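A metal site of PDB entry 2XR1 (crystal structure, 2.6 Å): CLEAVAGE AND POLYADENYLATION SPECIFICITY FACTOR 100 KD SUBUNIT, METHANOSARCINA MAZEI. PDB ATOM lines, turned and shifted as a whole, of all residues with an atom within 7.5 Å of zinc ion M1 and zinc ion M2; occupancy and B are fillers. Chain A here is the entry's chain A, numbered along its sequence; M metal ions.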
ATOM      1  N   VAL A 195       6.298  13.261  13.818  1.00  0.00           N
ATOM      2  CA  VAL A 195       5.086  12.499  13.599  1.00  0.00           C
ATOM      3  C   VAL A 195       4.259  12.756  14.847  1.00  0.00           C
ATOM      4  O   VAL A 195       4.791  12.655  15.974  1.00  0.00           O
ATOM      5  CB  VAL A 195       5.396  11.002  13.514  1.00  0.00           C
ATOM      6  CG1 VAL A 195       4.118  10.227  13.617  1.00  0.00           C
ATOM      7  CG2 VAL A 195       6.086  10.692  12.222  1.00  0.00           C
ATOM      8  N   GLY A 196       2.987  13.077  14.697  1.00  0.00           N
ATOM      9  CA  GLY A 196       2.178  13.316  15.875  1.00  0.00           C
ATOM     10  C   GLY A 196       1.631  14.733  15.900  1.00  0.00           C
ATOM     11  O   GLY A 196       2.242  15.674  15.413  1.00  0.00           O
ATOM     12  N   SER A 198      -0.625  16.396  14.400  1.00  0.00           N
ATOM     13  CA  SER A 198      -0.968  17.152  13.200  1.00  0.00           C
ATOM     14  C   SER A 198      -2.089  18.082  13.524  1.00  0.00           C
ATOM     15  O   SER A 198      -3.042  17.689  14.189  1.00  0.00           O
ATOM     16  CB  SER A 198      -1.410  16.228  12.058  1.00  0.00           C
ATOM     17  OG  SER A 198      -0.263  15.643  11.417  1.00  0.00           O
ATOM     18  N   ASP A 212      -7.086  18.902  10.651  1.00  0.00           N
ATOM     19  CA  ASP A 212      -6.636  17.942  11.672  1.00  0.00           C
ATOM     20  C   ASP A 212      -6.416  18.562  13.065  1.00  0.00           C
ATOM     21  O   ASP A 212      -6.224  19.771  13.209  1.00  0.00           O
ATOM     22  CB  ASP A 212      -5.421  17.123  11.190  1.00  0.00           C
ATOM     23  CG  ASP A 212      -5.787  16.087  10.059  1.00  0.00           C
ATOM     24  OD1 ASP A 212      -6.998  15.759   9.922  1.00  0.00           O
ATOM     25  OD2 ASP A 212      -4.864  15.604   9.306  1.00  0.00           O
ATOM     26  N   VAL A 217       2.237  11.433  19.427  1.00  0.00           N
ATOM     27  CA  VAL A 217       2.743  10.077  19.304  1.00  0.00           C
ATOM     28  C   VAL A 217       4.186  10.220  19.727  1.00  0.00           C
ATOM     29  O   VAL A 217       4.912  10.990  19.108  1.00  0.00           O
ATOM     30  CB  VAL A 217       2.718   9.615  17.826  1.00  0.00           C
ATOM     31  CG1 VAL A 217       3.501   8.324  17.673  1.00  0.00           C
ATOM     32  CG2 VAL A 217       1.274   9.484  17.308  1.00  0.00           C
ATOM     33  N   THR A 244      -8.789  14.518   8.087  1.00  0.00           N
ATOM     34  CA  THR A 244      -8.325  13.867   6.888  1.00  0.00           C
ATOM     35  C   THR A 244      -8.555  12.351   6.957  1.00  0.00           C
ATOM     36  O   THR A 244      -8.946  11.724   5.965  1.00  0.00           O
ATOM     37  CB  THR A 244      -6.821  14.126   6.676  1.00  0.00           C
ATOM     38  OG1 THR A 244      -6.082  13.513   7.731  1.00  0.00           O
ATOM     39  CG2 THR A 244      -6.487  15.614   6.690  1.00  0.00           C
ATOM     40  N   HIS A 245      -8.298  11.771   8.111  1.00  0.00           N
ATOM     41  CA  HIS A 245      -8.567  10.358   8.318  1.00  0.00           C
ATOM     42  C   HIS A 245      -8.645  10.052   9.805  1.00  0.00           C
ATOM     43  O   HIS A 245      -8.409  10.910  10.637  1.00  0.00           O
ATOM     44  CB  HIS A 245      -7.538   9.457   7.585  1.00  0.00           C
ATOM     45  CG  HIS A 245      -6.144   9.506   8.155  1.00  0.00           C
ATOM     46  ND1 HIS A 245      -5.329  10.594   8.012  1.00  0.00           N
ATOM     47  CD2 HIS A 245      -5.430   8.582   8.834  1.00  0.00           C
ATOM     48  CE1 HIS A 245      -4.174  10.345   8.592  1.00  0.00           C
ATOM     49  NE2 HIS A 245      -4.194   9.126   9.093  1.00  0.00           N
ATOM     50  N   ALA A 246      -9.009   8.818  10.143  1.00  0.00           N
ATOM     51  CA  ALA A 246      -9.501   8.526  11.472  1.00  0.00           C
ATOM     52  C   ALA A 246      -8.406   8.293  12.510  1.00  0.00           C
ATOM     53  O   ALA A 246      -8.698   8.153  13.699  1.00  0.00           O
ATOM     54  CB  ALA A 246     -10.436   7.357  11.410  1.00  0.00           C
ATOM     55  N   HIS A 247      -7.155   8.230  12.100  1.00  0.00           N
ATOM     56  CA  HIS A 247      -6.081   7.963  13.039  1.00  0.00           C
ATOM     57  C   HIS A 247      -6.047   8.990  14.164  1.00  0.00           C
ATOM     58  O   HIS A 247      -6.215  10.190  13.929  1.00  0.00           O
ATOM     59  CB  HIS A 247      -4.717   7.943  12.330  1.00  0.00           C
ATOM     60  CG  HIS A 247      -4.403   6.659  11.657  1.00  0.00           C
ATOM     61  ND1 HIS A 247      -3.578   6.582  10.558  1.00  0.00           N
ATOM     62  CD2 HIS A 247      -4.784   5.388  11.946  1.00  0.00           C
ATOM     63  CE1 HIS A 247      -3.455   5.315  10.192  1.00  0.00           C
ATOM     64  NE2 HIS A 247      -4.193   4.578  11.008  1.00  0.00           N
ATOM     65  N   LEU A 248      -5.786   8.502  15.377  1.00  0.00           N
ATOM     66  CA  LEU A 248      -5.729   9.357  16.570  1.00  0.00           C
ATOM     67  C   LEU A 248      -4.780  10.536  16.454  1.00  0.00           C
ATOM     68  O   LEU A 248      -5.039  11.600  17.024  1.00  0.00           O
ATOM     69  CB  LEU A 248      -5.386   8.539  17.824  1.00  0.00           C
ATOM     70  CG  LEU A 248      -6.664   8.038  18.488  1.00  0.00           C
ATOM     71  CD1 LEU A 248      -6.371   6.936  19.465  1.00  0.00           C
ATOM     72  CD2 LEU A 248      -7.451   9.194  19.125  1.00  0.00           C
ATOM     73  N   ASP A 249      -3.698  10.352  15.726  1.00  0.00           N
ATOM     74  CA  ASP A 249      -2.711  11.404  15.533  1.00  0.00           C
ATOM     75  C   ASP A 249      -3.225  12.419  14.550  1.00  0.00           C
ATOM     76  O   ASP A 249      -2.501  13.285  14.191  1.00  0.00           O
ATOM     77  CB  ASP A 249      -1.324  10.848  15.122  1.00  0.00           C
ATOM     78  CG  ASP A 249      -1.321  10.100  13.742  1.00  0.00           C
ATOM     79  OD1 ASP A 249      -2.095   9.145  13.569  1.00  0.00           O
ATOM     80  OD2 ASP A 249      -0.489  10.435  12.845  1.00  0.00           O
ATOM     81  N   HIS A 250      -4.487  12.347  14.135  1.00  0.00           N
ATOM     82  CA  HIS A 250      -5.106  13.418  13.305  1.00  0.00           C
ATOM     83  C   HIS A 250      -6.440  13.934  13.761  1.00  0.00           C
ATOM     84  O   HIS A 250      -6.773  15.049  13.368  1.00  0.00           O
ATOM     85  CB  HIS A 250      -5.258  12.942  11.874  1.00  0.00           C
ATOM     86  CG  HIS A 250      -3.955  12.604  11.252  1.00  0.00           C
ATOM     87  ND1 HIS A 250      -3.336  13.412  10.328  1.00  0.00           N
ATOM     88  CD2 HIS A 250      -3.107  11.567  11.492  1.00  0.00           C
ATOM     89  CE1 HIS A 250      -2.172  12.869  10.000  1.00  0.00           C
ATOM     90  NE2 HIS A 250      -2.013  11.751  10.689  1.00  0.00           N
ATOM     91  N   HIS A 332      -4.676   5.313   2.297  1.00  0.00           N
ATOM     92  CA  HIS A 332      -3.955   5.104   3.564  1.00  0.00           C
ATOM     93  C   HIS A 332      -4.779   4.204   4.480  1.00  0.00           C
ATOM     94  O   HIS A 332      -4.344   3.119   4.833  1.00  0.00           O
ATOM     95  CB  HIS A 332      -3.686   6.463   4.212  1.00  0.00           C
ATOM     96  CG  HIS A 332      -3.052   6.410   5.572  1.00  0.00           C
ATOM     97  ND1 HIS A 332      -1.837   5.808   5.807  1.00  0.00           N
ATOM     98  CD2 HIS A 332      -3.447   6.937   6.757  1.00  0.00           C
ATOM     99  CE1 HIS A 332      -1.525   5.945   7.094  1.00  0.00           C
ATOM    100  NE2 HIS A 332      -2.475   6.642   7.679  1.00  0.00           N
ATOM    101  N   ILE A 333      -5.959   4.639   4.847  1.00  0.00           N
ATOM    102  CA  ILE A 333      -6.916   3.767   5.527  1.00  0.00           C
ATOM    103  C   ILE A 333      -8.331   4.077   5.048  1.00  0.00           C
ATOM    104  O   ILE A 333      -8.589   5.084   4.366  1.00  0.00           O
ATOM    105  CB  ILE A 333      -6.889   3.907   7.070  1.00  0.00           C
ATOM    106  CG1 ILE A 333      -7.325   5.318   7.511  1.00  0.00           C
ATOM    107  CG2 ILE A 333      -5.529   3.530   7.619  1.00  0.00           C
ATOM    108  CD1 ILE A 333      -7.567   5.463   8.977  1.00  0.00           C
ATOM    109  N   SER A 336      -9.617   7.484   4.162  1.00  0.00           N
ATOM    110  CA  SER A 336      -8.579   8.497   4.208  1.00  0.00           C
ATOM    111  C   SER A 336      -8.723   9.421   3.037  1.00  0.00           C
ATOM    112  O   SER A 336      -9.021   8.985   1.922  1.00  0.00           O
ATOM    113  CB  SER A 336      -7.182   7.906   4.254  1.00  0.00           C
ATOM    114  OG  SER A 336      -6.817   7.218   3.074  1.00  0.00           O
ATOM    115  N   GLY A 354      -2.668  14.823   3.806  1.00  0.00           N
ATOM    116  CA  GLY A 354      -2.813  13.922   4.944  1.00  0.00           C
ATOM    117  C   GLY A 354      -1.856  12.756   4.767  1.00  0.00           C
ATOM    118  O   GLY A 354      -0.813  12.884   4.092  1.00  0.00           O
ATOM    119  N   ASP A 355      -2.174  11.617   5.370  1.00  0.00           N
ATOM    120  CA  ASP A 355      -1.352  10.426   5.192  1.00  0.00           C
ATOM    121  C   ASP A 355      -1.865   9.757   3.921  1.00  0.00           C
ATOM    122  O   ASP A 355      -3.083   9.768   3.680  1.00  0.00           O
ATOM    123  CB  ASP A 355      -1.450   9.507   6.414  1.00  0.00           C
ATOM    124  CG  ASP A 355      -0.817  10.122   7.711  1.00  0.00           C
ATOM    125  OD1 ASP A 355      -0.196  11.237   7.653  1.00  0.00           O
ATOM    126  OD2 ASP A 355      -0.968   9.484   8.788  1.00  0.00           O
ATOM    127  N   TYR A 356      -0.973   9.243   3.086  1.00  0.00           N
ATOM    128  CA  TYR A 356      -1.373   8.652   1.798  1.00  0.00           C
ATOM    129  C   TYR A 356      -0.459   7.573   1.220  1.00  0.00           C
ATOM    130  O   TYR A 356       0.677   7.433   1.616  1.00  0.00           O
ATOM    131  CB  TYR A 356      -1.505   9.752   0.749  1.00  0.00           C
ATOM    132  CG  TYR A 356      -0.210  10.410   0.304  1.00  0.00           C
ATOM    133  CD1 TYR A 356       0.274  11.517   0.952  1.00  0.00           C
ATOM    134  CD2 TYR A 356       0.485   9.943  -0.793  1.00  0.00           C
ATOM    135  CE1 TYR A 356       1.440  12.139   0.533  1.00  0.00           C
ATOM    136  CE2 TYR A 356       1.671  10.536  -1.220  1.00  0.00           C
ATOM    137  CZ  TYR A 356       2.142  11.632  -0.555  1.00  0.00           C
ATOM    138  OH  TYR A 356       3.303  12.241  -0.975  1.00  0.00           O
ATOM    139  N   GLU A 380       2.679  14.739   3.532  1.00  0.00           N
ATOM    140  CA  GLU A 380       3.360  13.974   4.586  1.00  0.00           C
ATOM    141  C   GLU A 380       4.719  13.539   4.133  1.00  0.00           C
ATOM    142  O   GLU A 380       4.991  13.524   2.920  1.00  0.00           O
ATOM    143  CB  GLU A 380       2.600  12.719   4.964  1.00  0.00           C
ATOM    144  CG  GLU A 380       2.577  11.627   3.900  1.00  0.00           C
ATOM    145  CD  GLU A 380       2.680  10.220   4.492  1.00  0.00           C
ATOM    146  OE1 GLU A 380       3.644   9.941   5.248  1.00  0.00           O
ATOM    147  OE2 GLU A 380       1.784   9.401   4.212  1.00  0.00           O
ATOM    148  N   THR A 382       6.474  10.665   6.100  1.00  0.00           N
ATOM    149  CA  THR A 382       6.830   9.645   7.101  1.00  0.00           C
ATOM    150  C   THR A 382       8.024   8.808   6.690  1.00  0.00           C
ATOM    151  O   THR A 382       8.932   8.567   7.491  1.00  0.00           O
ATOM    152  CB  THR A 382       5.686   8.680   7.438  1.00  0.00           C
ATOM    153  OG1 THR A 382       4.425   9.372   7.534  1.00  0.00           O
ATOM    154  CG2 THR A 382       6.004   7.941   8.749  1.00  0.00           C
ATOM    155  N   VAL A 421      -7.465   0.413  13.360  1.00  0.00           N
ATOM    156  CA  VAL A 421      -7.638   0.527  11.933  1.00  0.00           C
ATOM    157  C   VAL A 421      -6.365   0.949  11.219  1.00  0.00           C
ATOM    158  O   VAL A 421      -5.716   1.921  11.585  1.00  0.00           O
ATOM    159  CB  VAL A 421      -8.736   1.519  11.585  1.00  0.00           C
ATOM    160  CG1 VAL A 421      -8.444   2.827  12.195  1.00  0.00           C
ATOM    161  CG2 VAL A 421      -8.859   1.606  10.086  1.00  0.00           C
ATOM    162  N   TYR A 539       6.206   1.488  10.697  1.00  0.00           N
ATOM    163  CA  TYR A 539       7.160   2.300  11.456  1.00  0.00           C
ATOM    164  C   TYR A 539       6.715   2.499  12.907  1.00  0.00           C
ATOM    165  O   TYR A 539       5.519   2.438  13.226  1.00  0.00           O
ATOM    166  CB  TYR A 539       7.422   3.672  10.803  1.00  0.00           C
ATOM    167  CG  TYR A 539       6.341   4.672  11.083  1.00  0.00           C
ATOM    168  CD1 TYR A 539       5.148   4.611  10.396  1.00  0.00           C
ATOM    169  CD2 TYR A 539       6.513   5.680  12.021  1.00  0.00           C
ATOM    170  CE1 TYR A 539       4.115   5.517  10.645  1.00  0.00           C
ATOM    171  CE2 TYR A 539       5.499   6.608  12.278  1.00  0.00           C
ATOM    172  CZ  TYR A 539       4.290   6.515  11.586  1.00  0.00           C
ATOM    173  OH  TYR A 539       3.254   7.400  11.813  1.00  0.00           O
ATOM    174  N   SER A 581       2.406  -0.310   6.762  1.00  0.00           N
ATOM    175  CA  SER A 581       2.221   0.956   7.449  1.00  0.00           C
ATOM    176  C   SER A 581       1.080   1.719   6.844  1.00  0.00           C
ATOM    177  O   SER A 581       0.462   2.533   7.538  1.00  0.00           O
ATOM    178  CB  SER A 581       3.493   1.791   7.359  1.00  0.00           C
ATOM    179  OG  SER A 581       3.782   2.102   6.009  1.00  0.00           O
ATOM    180  N   GLY A 582       0.791   1.478   5.561  1.00  0.00           N
ATOM    181  CA  GLY A 582      -0.209   2.256   4.824  1.00  0.00           C
ATOM    182  C   GLY A 582       0.294   3.608   4.329  1.00  0.00           C
ATOM    183  O   GLY A 582      -0.493   4.406   3.866  1.00  0.00           O
ATOM    184  N   HIS A 583       1.605   3.863   4.402  1.00  0.00           N
ATOM    185  CA  HIS A 583       2.234   5.068   3.857  1.00  0.00           C
ATOM    186  C   HIS A 583       3.049   4.815   2.603  1.00  0.00           C
ATOM    187  O   HIS A 583       3.676   3.770   2.460  1.00  0.00           O
ATOM    188  CB  HIS A 583       3.213   5.670   4.863  1.00  0.00           C
ATOM    189  CG  HIS A 583       2.565   6.206   6.091  1.00  0.00           C
ATOM    190  ND1 HIS A 583       2.095   7.494   6.174  1.00  0.00           N
ATOM    191  CD2 HIS A 583       2.323   5.643   7.292  1.00  0.00           C
ATOM    192  CE1 HIS A 583       1.567   7.691   7.373  1.00  0.00           C
ATOM    193  NE2 HIS A 583       1.708   6.593   8.073  1.00  0.00           N
ATOM    194  N   GLU A 606       5.728  17.663   6.066  1.00  0.00           N
ATOM    195  CA  GLU A 606       5.338  17.522   7.465  1.00  0.00           C
ATOM    196  C   GLU A 606       5.127  16.044   7.769  1.00  0.00           C
ATOM    197  O   GLU A 606       5.255  15.224   6.890  1.00  0.00           O
ATOM    198  CB  GLU A 606       4.078  18.334   7.728  1.00  0.00           C
ATOM    199  CG  GLU A 606       2.960  18.130   6.688  1.00  0.00           C
ATOM    200  CD  GLU A 606       1.933  17.047   7.035  1.00  0.00           C
ATOM    201  OE1 GLU A 606       1.595  16.846   8.240  1.00  0.00           O
ATOM    202  OE2 GLU A 606       1.462  16.420   6.080  1.00  0.00           O
ATOM    203  N   HIS A 607       4.819  15.692   8.998  1.00  0.00           N
ATOM    204  CA  HIS A 607       4.538  14.307   9.356  1.00  0.00           C
ATOM    205  C   HIS A 607       5.700  13.350   9.035  1.00  0.00           C
ATOM    206  O   HIS A 607       5.606  12.433   8.219  1.00  0.00           O
ATOM    207  CB  HIS A 607       3.253  13.874   8.677  1.00  0.00           C
ATOM    208  CG  HIS A 607       2.629  12.652   9.262  1.00  0.00           C
ATOM    209  ND1 HIS A 607       3.095  11.394   9.013  1.00  0.00           N
ATOM    210  CD2 HIS A 607       1.544  12.502  10.054  1.00  0.00           C
ATOM    211  CE1 HIS A 607       2.331  10.502   9.629  1.00  0.00           C
ATOM    212  NE2 HIS A 607       1.374  11.155  10.261  1.00  0.00           N
HETATM  213 ZN    ZN M   1      -2.556   7.956   9.597  1.00  0.00          ZN
HETATM  214 ZN    ZN M   2      -0.570  10.189  10.610  1.00  0.00          ZN
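Within 4 Å of zinc ion M1: His 245, His 247, His 250, His 332 and Asp 355.
Four residues have an atom within 4 Å of zinc ion M2: Asp 249, His 250, Asp 355 and His 607. The nearest printed residue that does not touch zinc ion M2 is His 245 (4.1 Å).
Zinc ion M1 is bound by a ring nitrogen (ND1) of His 247, a ring nitrogen (NE2) of His 245, a ring nitrogen (NE2) of His 332 and the side-chain carboxylate (OD2) of Asp 355.
Zinc ion M2 is bound by OD2 of Asp 355 (2.0 Å), NE2 of His 250 (2.1 Å), NE2 of His 607 (2.2 Å) and OD2 of Asp 249 (2.2 Å). Zinc ion M2 has four donor atoms within binding distance.
The side-chain carboxylate (OD2) of Asp 212 sits at hydrogen-bond distance from a ring nitrogen (ND1) of His 250 (2.9 Å). The backbone carbonyl oxygen (O) of Gly 582 lies within hydrogen-bond range of a ring nitrogen (ND1) of His 332 (2.7 Å). The side-chain hydroxyl (OG1) of Thr 382 is in hydrogen-bond range of a ring nitrogen (ND1) of His 607 (2.8 Å). A ring nitrogen (NE2) of His 247 lies within hydrogen-bond range of the backbone carbonyl oxygen of Val 421, 3.1 Å away. The backbone NH (N) of His 332 lies within hydrogen-bond range of the side-chain hydroxyl (OG) of Ser 336, 3.0 Å away. A ring nitrogen (ND1) of His 245 sits at hydrogen-bond distance from the side-chain hydroxyl of Thr 244 (3.0 Å).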
